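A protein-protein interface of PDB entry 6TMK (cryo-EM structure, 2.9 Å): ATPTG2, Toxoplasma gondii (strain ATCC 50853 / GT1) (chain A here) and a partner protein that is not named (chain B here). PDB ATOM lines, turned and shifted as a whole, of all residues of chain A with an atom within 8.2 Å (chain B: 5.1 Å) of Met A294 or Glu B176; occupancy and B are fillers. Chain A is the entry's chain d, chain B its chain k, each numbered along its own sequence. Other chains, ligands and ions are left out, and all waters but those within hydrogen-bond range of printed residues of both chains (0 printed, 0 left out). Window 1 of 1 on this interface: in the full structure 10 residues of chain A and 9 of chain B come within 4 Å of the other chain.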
ATOM      1  N   ASN A 274     -12.278 -11.937  -9.208  1.00  0.00           N
ATOM      2  CA  ASN A 274     -12.501 -10.543  -9.549  1.00  0.00           C
ATOM      3  C   ASN A 274     -12.816 -10.462 -11.036  1.00  0.00           C
ATOM      4  O   ASN A 274     -12.794 -11.466 -11.752  1.00  0.00           O
ATOM      5  CB  ASN A 274     -11.294  -9.671  -9.183  1.00  0.00           C
ATOM      6  CG  ASN A 274     -10.037 -10.078  -9.904  1.00  0.00           C
ATOM      7  OD1 ASN A 274      -9.850  -9.768 -11.078  1.00  0.00           O
ATOM      8  ND2 ASN A 274      -9.157 -10.767  -9.200  1.00  0.00           N
ATOM      9  N   LEU A 276     -11.393  -7.627 -12.821  1.00  0.00           N
ATOM     10  CA  LEU A 276     -10.519  -6.524 -13.167  1.00  0.00           C
ATOM     11  C   LEU A 276      -9.200  -6.971 -13.770  1.00  0.00           C
ATOM     12  O   LEU A 276      -8.489  -6.139 -14.343  1.00  0.00           O
ATOM     13  CB  LEU A 276     -10.228  -5.676 -11.922  1.00  0.00           C
ATOM     14  CG  LEU A 276     -11.401  -5.460 -10.974  1.00  0.00           C
ATOM     15  CD1 LEU A 276     -10.907  -4.770  -9.748  1.00  0.00           C
ATOM     16  CD2 LEU A 276     -12.515  -4.669 -11.622  1.00  0.00           C
ATOM     17  N   SER A 277      -8.850  -8.248 -13.657  1.00  0.00           N
ATOM     18  CA  SER A 277      -7.663  -8.790 -14.296  1.00  0.00           C
ATOM     19  C   SER A 277      -7.848  -9.035 -15.784  1.00  0.00           C
ATOM     20  O   SER A 277      -6.922  -9.531 -16.432  1.00  0.00           O
ATOM     21  CB  SER A 277      -7.265 -10.104 -13.626  1.00  0.00           C
ATOM     22  OG  SER A 277      -8.326 -11.040 -13.681  1.00  0.00           O
ATOM     23  N   GLY A 278      -9.005  -8.702 -16.343  1.00  0.00           N
ATOM     24  CA  GLY A 278      -9.241  -8.964 -17.746  1.00  0.00           C
ATOM     25  C   GLY A 278     -10.374  -8.131 -18.292  1.00  0.00           C
ATOM     26  O   GLY A 278     -11.071  -7.422 -17.564  1.00  0.00           O
ATOM     27  N   ASP A 288     -10.318 -11.929 -25.632  1.00  0.00           N
ATOM     28  CA  ASP A 288      -9.961 -12.916 -24.627  1.00  0.00           C
ATOM     29  C   ASP A 288      -9.612 -12.235 -23.311  1.00  0.00           C
ATOM     30  O   ASP A 288      -8.770 -11.334 -23.268  1.00  0.00           O
ATOM     31  CB  ASP A 288      -8.785 -13.755 -25.114  1.00  0.00           C
ATOM     32  CG  ASP A 288      -8.681 -15.086 -24.404  1.00  0.00           C
ATOM     33  OD1 ASP A 288      -9.091 -15.171 -23.228  1.00  0.00           O
ATOM     34  OD2 ASP A 288      -8.172 -16.046 -25.017  1.00  0.00           O
ATOM     35  N   ASN A 289     -10.261 -12.677 -22.236  1.00  0.00           N
ATOM     36  CA  ASN A 289      -9.994 -12.119 -20.915  1.00  0.00           C
ATOM     37  C   ASN A 289      -8.582 -12.444 -20.448  1.00  0.00           C
ATOM     38  O   ASN A 289      -7.922 -11.610 -19.820  1.00  0.00           O
ATOM     39  CB  ASN A 289     -11.030 -12.615 -19.912  1.00  0.00           C
ATOM     40  CG  ASN A 289     -11.206 -14.113 -19.947  1.00  0.00           C
ATOM     41  OD1 ASN A 289     -11.253 -14.720 -21.013  1.00  0.00           O
ATOM     42  ND2 ASN A 289     -11.303 -14.717 -18.776  1.00  0.00           N
ATOM     43  N   LYS A 290      -8.107 -13.653 -20.730  1.00  0.00           N
ATOM     44  CA  LYS A 290      -6.781 -14.064 -20.308  1.00  0.00           C
ATOM     45  C   LYS A 290      -5.728 -13.553 -21.279  1.00  0.00           C
ATOM     46  O   LYS A 290      -6.001 -13.314 -22.458  1.00  0.00           O
ATOM     47  CB  LYS A 290      -6.689 -15.585 -20.212  1.00  0.00           C
ATOM     48  CG  LYS A 290      -7.683 -16.212 -19.270  1.00  0.00           C
ATOM     49  CD  LYS A 290      -7.416 -15.819 -17.846  1.00  0.00           C
ATOM     50  CE  LYS A 290      -8.432 -16.420 -16.920  1.00  0.00           C
ATOM     51  NZ  LYS A 290      -8.454 -15.700 -15.626  1.00  0.00           N
ATOM     52  N   ASN A 291      -4.514 -13.385 -20.770  1.00  0.00           N
ATOM     53  CA  ASN A 291      -3.424 -12.872 -21.577  1.00  0.00           C
ATOM     54  C   ASN A 291      -2.663 -14.018 -22.242  1.00  0.00           C
ATOM     55  O   ASN A 291      -2.961 -15.199 -22.053  1.00  0.00           O
ATOM     56  CB  ASN A 291      -2.500 -12.010 -20.724  1.00  0.00           C
ATOM     57  CG  ASN A 291      -1.890 -12.769 -19.579  1.00  0.00           C
ATOM     58  OD1 ASN A 291      -2.595 -13.331 -18.744  1.00  0.00           O
ATOM     59  ND2 ASN A 291      -0.573 -12.778 -19.519  1.00  0.00           N
ATOM     60  N   ALA A 292      -1.650 -13.654 -23.026  1.00  0.00           N
ATOM     61  CA  ALA A 292      -1.051 -14.585 -23.973  1.00  0.00           C
ATOM     62  C   ALA A 292      -0.344 -15.752 -23.293  1.00  0.00           C
ATOM     63  O   ALA A 292      -0.340 -16.864 -23.832  1.00  0.00           O
ATOM     64  CB  ALA A 292      -0.081 -13.838 -24.883  1.00  0.00           C
ATOM     65  N   LEU A 293       0.261 -15.530 -22.129  1.00  0.00           N
ATOM     66  CA  LEU A 293       1.067 -16.563 -21.491  1.00  0.00           C
ATOM     67  C   LEU A 293       0.237 -17.657 -20.835  1.00  0.00           C
ATOM     68  O   LEU A 293       0.746 -18.763 -20.639  1.00  0.00           O
ATOM     69  CB  LEU A 293       1.986 -15.940 -20.445  1.00  0.00           C
ATOM     70  CG  LEU A 293       2.912 -14.837 -20.942  1.00  0.00           C
ATOM     71  CD1 LEU A 293       3.632 -14.214 -19.773  1.00  0.00           C
ATOM     72  CD2 LEU A 293       3.890 -15.373 -21.952  1.00  0.00           C
ATOM     73  N   MET A 294      -1.016 -17.380 -20.497  1.00  0.00           N
ATOM     74  CA  MET A 294      -1.879 -18.328 -19.813  1.00  0.00           C
ATOM     75  C   MET A 294      -3.054 -18.786 -20.659  1.00  0.00           C
ATOM     76  O   MET A 294      -3.809 -19.658 -20.224  1.00  0.00           O
ATOM     77  CB  MET A 294      -2.403 -17.713 -18.515  1.00  0.00           C
ATOM     78  CG  MET A 294      -2.814 -16.294 -18.639  1.00  0.00           C
ATOM     79  SD  MET A 294      -3.759 -15.749 -17.210  1.00  0.00           S
ATOM     80  CE  MET A 294      -2.494 -15.851 -15.957  1.00  0.00           C
ATOM     81  N   ARG A 295      -3.228 -18.225 -21.849  1.00  0.00           N
ATOM     82  CA  ARG A 295      -4.180 -18.770 -22.809  1.00  0.00           C
ATOM     83  C   ARG A 295      -3.964 -20.242 -23.119  1.00  0.00           C
ATOM     84  O   ARG A 295      -4.963 -20.970 -23.241  1.00  0.00           O
ATOM     85  CB  ARG A 295      -4.124 -17.935 -24.093  1.00  0.00           C
ATOM     86  CG  ARG A 295      -5.070 -16.779 -24.079  1.00  0.00           C
ATOM     87  CD  ARG A 295      -4.832 -15.802 -25.201  1.00  0.00           C
ATOM     88  NE  ARG A 295      -4.985 -14.430 -24.739  1.00  0.00           N
ATOM     89  CZ  ARG A 295      -4.462 -13.370 -25.334  1.00  0.00           C
ATOM     90  NH1 ARG A 295      -3.746 -13.499 -26.431  1.00  0.00           N
ATOM     91  NH2 ARG A 295      -4.660 -12.174 -24.819  1.00  0.00           N
ATOM     92  N   PRO A 296      -2.739 -20.745 -23.267  1.00  0.00           N
ATOM     93  CA  PRO A 296      -2.567 -22.191 -23.452  1.00  0.00           C
ATOM     94  C   PRO A 296      -3.008 -23.021 -22.256  1.00  0.00           C
ATOM     95  O   PRO A 296      -3.279 -24.215 -22.420  1.00  0.00           O
ATOM     96  CB  PRO A 296      -1.063 -22.326 -23.720  1.00  0.00           C
ATOM     97  CG  PRO A 296      -0.667 -21.019 -24.270  1.00  0.00           C
ATOM     98  CD  PRO A 296      -1.504 -20.009 -23.570  1.00  0.00           C
ATOM     99  N   ALA A 297      -3.080 -22.436 -21.064  1.00  0.00           N
ATOM    100  CA  ALA A 297      -3.450 -23.140 -19.841  1.00  0.00           C
ATOM    101  C   ALA A 297      -4.780 -22.646 -19.274  1.00  0.00           C
ATOM    102  O   ALA A 297      -4.951 -22.531 -18.062  1.00  0.00           O
ATOM    103  CB  ALA A 297      -2.356 -23.001 -18.797  1.00  0.00           C
ATOM    104  N   ARG A 298      -5.743 -22.365 -20.153  1.00  0.00           N
ATOM    105  CA  ARG A 298      -7.039 -21.863 -19.715  1.00  0.00           C
ATOM    106  C   ARG A 298      -7.787 -22.880 -18.869  1.00  0.00           C
ATOM    107  O   ARG A 298      -8.556 -22.505 -17.981  1.00  0.00           O
ATOM    108  CB  ARG A 298      -7.862 -21.493 -20.944  1.00  0.00           C
ATOM    109  CG  ARG A 298      -9.099 -20.674 -20.696  1.00  0.00           C
ATOM    110  CD  ARG A 298      -9.966 -20.713 -21.921  1.00  0.00           C
ATOM    111  NE  ARG A 298      -9.219 -20.274 -23.089  1.00  0.00           N
ATOM    112  CZ  ARG A 298      -8.904 -19.010 -23.340  1.00  0.00           C
ATOM    113  NH1 ARG A 298      -9.288 -18.051 -22.514  1.00  0.00           N
ATOM    114  NH2 ARG A 298      -8.206 -18.704 -24.419  1.00  0.00           N
ATOM    115  N   MET A 299      -7.569 -24.165 -19.131  1.00  0.00           N
ATOM    116  CA  MET A 299      -8.235 -25.222 -18.382  1.00  0.00           C
ATOM    117  C   MET A 299      -7.941 -25.141 -16.891  1.00  0.00           C
ATOM    118  O   MET A 299      -8.748 -25.594 -16.073  1.00  0.00           O
ATOM    119  CB  MET A 299      -7.798 -26.569 -18.929  1.00  0.00           C
ATOM    120  CG  MET A 299      -8.646 -27.724 -18.513  1.00  0.00           C
ATOM    121  SD  MET A 299      -7.812 -29.268 -18.875  1.00  0.00           S
ATOM    122  CE  MET A 299      -9.208 -30.365 -18.823  1.00  0.00           C
ATOM    123  N   MET A 300      -6.808 -24.558 -16.517  1.00  0.00           N
ATOM    124  CA  MET A 300      -6.393 -24.494 -15.126  1.00  0.00           C
ATOM    125  C   MET A 300      -7.073 -23.380 -14.350  1.00  0.00           C
ATOM    126  O   MET A 300      -7.001 -23.372 -13.119  1.00  0.00           O
ATOM    127  CB  MET A 300      -4.886 -24.310 -15.070  1.00  0.00           C
ATOM    128  CG  MET A 300      -4.124 -25.548 -15.462  1.00  0.00           C
ATOM    129  SD  MET A 300      -2.394 -25.214 -15.805  1.00  0.00           S
ATOM    130  CE  MET A 300      -1.910 -24.606 -14.212  1.00  0.00           C
ATOM    131  N   PHE A 301      -7.706 -22.436 -15.036  1.00  0.00           N
ATOM    132  CA  PHE A 301      -8.425 -21.337 -14.414  1.00  0.00           C
ATOM    133  C   PHE A 301      -9.934 -21.552 -14.450  1.00  0.00           C
ATOM    134  O   PHE A 301     -10.695 -20.587 -14.554  1.00  0.00           O
ATOM    135  CB  PHE A 301      -8.031 -20.035 -15.100  1.00  0.00           C
ATOM    136  CG  PHE A 301      -6.552 -19.846 -15.195  1.00  0.00           C
ATOM    137  CD1 PHE A 301      -5.837 -19.375 -14.117  1.00  0.00           C
ATOM    138  CD2 PHE A 301      -5.870 -20.175 -16.345  1.00  0.00           C
ATOM    139  CE1 PHE A 301      -4.480 -19.218 -14.193  1.00  0.00           C
ATOM    140  CE2 PHE A 301      -4.514 -20.019 -16.421  1.00  0.00           C
ATOM    141  CZ  PHE A 301      -3.818 -19.540 -15.343  1.00  0.00           C
ATOM    142  N   SER B 172      -3.901 -11.658  -4.125  1.00  0.00           N
ATOM    143  CA  SER B 172      -4.435 -11.556  -5.476  1.00  0.00           C
ATOM    144  C   SER B 172      -3.357 -11.356  -6.532  1.00  0.00           C
ATOM    145  O   SER B 172      -3.293 -12.123  -7.493  1.00  0.00           O
ATOM    146  CB  SER B 172      -5.448 -10.412  -5.544  1.00  0.00           C
ATOM    147  OG  SER B 172      -6.614 -10.733  -4.807  1.00  0.00           O
ATOM    148  N   VAL B 173      -2.502 -10.347  -6.385  1.00  0.00           N
ATOM    149  CA  VAL B 173      -1.600 -10.020  -7.485  1.00  0.00           C
ATOM    150  C   VAL B 173      -0.404 -10.966  -7.495  1.00  0.00           C
ATOM    151  O   VAL B 173       0.012 -11.456  -8.554  1.00  0.00           O
ATOM    152  CB  VAL B 173      -1.172  -8.544  -7.402  1.00  0.00           C
ATOM    153  CG1 VAL B 173      -2.385  -7.651  -7.240  1.00  0.00           C
ATOM    154  CG2 VAL B 173      -0.193  -8.320  -6.281  1.00  0.00           C
ATOM    155  N   PHE B 174       0.156 -11.264  -6.323  1.00  0.00           N
ATOM    156  CA  PHE B 174       1.188 -12.287  -6.273  1.00  0.00           C
ATOM    157  C   PHE B 174       0.609 -13.644  -6.645  1.00  0.00           C
ATOM    158  O   PHE B 174       1.306 -14.483  -7.227  1.00  0.00           O
ATOM    159  CB  PHE B 174       1.811 -12.343  -4.880  1.00  0.00           C
ATOM    160  CG  PHE B 174       2.364 -11.028  -4.408  1.00  0.00           C
ATOM    161  CD1 PHE B 174       2.502 -10.771  -3.057  1.00  0.00           C
ATOM    162  CD2 PHE B 174       2.686 -10.030  -5.308  1.00  0.00           C
ATOM    163  CE1 PHE B 174       2.994  -9.563  -2.613  1.00  0.00           C
ATOM    164  CE2 PHE B 174       3.163  -8.813  -4.870  1.00  0.00           C
ATOM    165  CZ  PHE B 174       3.327  -8.582  -3.519  1.00  0.00           C
ATOM    166  N   GLY B 175      -0.667 -13.865  -6.330  1.00  0.00           N
ATOM    167  CA  GLY B 175      -1.352 -15.045  -6.820  1.00  0.00           C
ATOM    168  C   GLY B 175      -1.392 -15.108  -8.333  1.00  0.00           C
ATOM    169  O   GLY B 175      -1.173 -16.164  -8.924  1.00  0.00           O
ATOM    170  N   GLU B 176      -1.691 -13.979  -8.975  1.00  0.00           N
ATOM    171  CA  GLU B 176      -1.698 -13.920 -10.431  1.00  0.00           C
ATOM    172  C   GLU B 176      -0.318 -14.226 -10.992  1.00  0.00           C
ATOM    173  O   GLU B 176      -0.189 -14.894 -12.025  1.00  0.00           O
ATOM    174  CB  GLU B 176      -2.175 -12.542 -10.887  1.00  0.00           C
ATOM    175  CG  GLU B 176      -2.703 -12.484 -12.305  1.00  0.00           C
ATOM    176  CD  GLU B 176      -4.160 -12.893 -12.413  1.00  0.00           C
ATOM    177  OE1 GLU B 176      -4.965 -12.450 -11.570  1.00  0.00           O
ATOM    178  OE2 GLU B 176      -4.502 -13.650 -13.345  1.00  0.00           O
ATOM    179  N   VAL B 177       0.727 -13.751 -10.321  1.00  0.00           N
ATOM    180  CA  VAL B 177       2.087 -14.030 -10.775  1.00  0.00           C
ATOM    181  C   VAL B 177       2.378 -15.526 -10.676  1.00  0.00           C
ATOM    182  O   VAL B 177       2.901 -16.147 -11.615  1.00  0.00           O
ATOM    183  CB  VAL B 177       3.097 -13.202  -9.963  1.00  0.00           C
ATOM    184  CG1 VAL B 177       4.508 -13.635 -10.267  1.00  0.00           C
ATOM    185  CG2 VAL B 177       2.919 -11.731 -10.247  1.00  0.00           C
ATOM    186  N   MET B 178       2.043 -16.123  -9.532  1.00  0.00           N
ATOM    187  CA  MET B 178       2.204 -17.561  -9.368  1.00  0.00           C
ATOM    188  C   MET B 178       1.404 -18.321 -10.414  1.00  0.00           C
ATOM    189  O   MET B 178       1.839 -19.370 -10.898  1.00  0.00           O
ATOM    190  CB  MET B 178       1.758 -17.975  -7.969  1.00  0.00           C
ATOM    191  CG  MET B 178       2.568 -17.375  -6.850  1.00  0.00           C
ATOM    192  SD  MET B 178       4.257 -17.981  -6.808  1.00  0.00           S
ATOM    193  CE  MET B 178       5.140 -16.439  -6.687  1.00  0.00           C
ATOM    194  N   LYS B 179       0.227 -17.810 -10.763  1.00  0.00           N
ATOM    195  CA  LYS B 179      -0.612 -18.464 -11.756  1.00  0.00           C
ATOM    196  C   LYS B 179       0.033 -18.417 -13.130  1.00  0.00           C
ATOM    197  O   LYS B 179      -0.024 -19.391 -13.886  1.00  0.00           O
ATOM    198  CB  LYS B 179      -1.987 -17.802 -11.779  1.00  0.00           C
ATOM    199  CG  LYS B 179      -2.883 -18.230 -10.634  1.00  0.00           C
ATOM    200  CD  LYS B 179      -4.219 -17.503 -10.643  1.00  0.00           C
ATOM    201  CE  LYS B 179      -5.094 -17.938  -9.475  1.00  0.00           C
ATOM    202  NZ  LYS B 179      -6.530 -18.152  -9.848  1.00  0.00           N
ATOM    203  N   LEU B 180       0.655 -17.289 -13.467  1.00  0.00           N
ATOM    204  CA  LEU B 180       1.433 -17.210 -14.696  1.00  0.00           C
ATOM    205  C   LEU B 180       2.528 -18.267 -14.714  1.00  0.00           C
ATOM    206  O   LEU B 180       2.720 -18.974 -15.712  1.00  0.00           O
ATOM    207  CB  LEU B 180       2.047 -15.821 -14.830  1.00  0.00           C
ATOM    208  CG  LEU B 180       1.175 -14.705 -15.379  1.00  0.00           C
ATOM    209  CD1 LEU B 180       1.870 -13.382 -15.156  1.00  0.00           C
ATOM    210  CD2 LEU B 180       0.908 -14.932 -16.849  1.00  0.00           C
ATOM    211  N   ALA B 183       1.080 -21.680 -15.246  1.00  0.00           N
ATOM    212  CA  ALA B 183       0.639 -21.866 -16.617  1.00  0.00           C
ATOM    213  C   ALA B 183       1.813 -22.110 -17.547  1.00  0.00           C
ATOM    214  O   ALA B 183       1.678 -22.831 -18.539  1.00  0.00           O
ATOM    215  CB  ALA B 183      -0.155 -20.644 -17.070  1.00  0.00           C
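The side-chain amide oxygen (OD1) of Asn A291 lies close to the side-chain sulfur (SD) of Met A294 (3.1 Å). The side-chain amide oxygen (OD1) of Asn A274 is in hydrogen-bond range of the backbone NH (N) of Ser A277 (3.2 Å). O of Asn A291 lies close to NE of Arg A295 (3.5 Å).
Glu B176 touches Ser A277 (OE1 to CB, 3.9 Å). Asn A291 touches Leu B180. Leu B180 touches Leu A293. Met A294 touches Glu B176 (CE to OE2, 3.96 Å). CE of Met A294 touches CD2 of Leu B180, at 3.6 Å. Ala B183 touches Met A294. CB of Ala B183 touches CB of Ala A297, 3.7 Å away. CE1 of Phe A301 touches CB of Lys B179, 3.7 Å away.
Gly A278 touches none of the printed residues of chain B. Printed residues of chain B within 4 Å of Asn A291: Leu B180 (3.7 Å). Of the printed residues of chain B, Leu A293 touches Leu B180. Pro A296 touches none of the printed residues of chain B. Printed residues of chain B within 4 Å of Ala A297: Ala B183 (3.7 Å). Of chain A, only Ser A277 (3.9 Å) and Met A294 (3.96 Å) come within 4 Å of Glu B176. Of the printed residues of chain A, Ala B183 touches Met A294 and Ala A297. The nearest residue of chain B that does not touch Met A294 is Lys B179 (4.6 Å). The nearest printed residue of chain A that does not touch Ala B183 is Leu A293 (4.1 Å).
Hydrophobic or aromatic side chains of chain B within 4 Å of the printed part of chain A: Leu B180 and Ala B183. Printed residues of chain A that touch a printed residue of chain B: Ser A277, Asn A291, Leu A293, Met A294, Ala A297 and Phe A301. Among the printed residues, 8 pairs touch across the chains.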
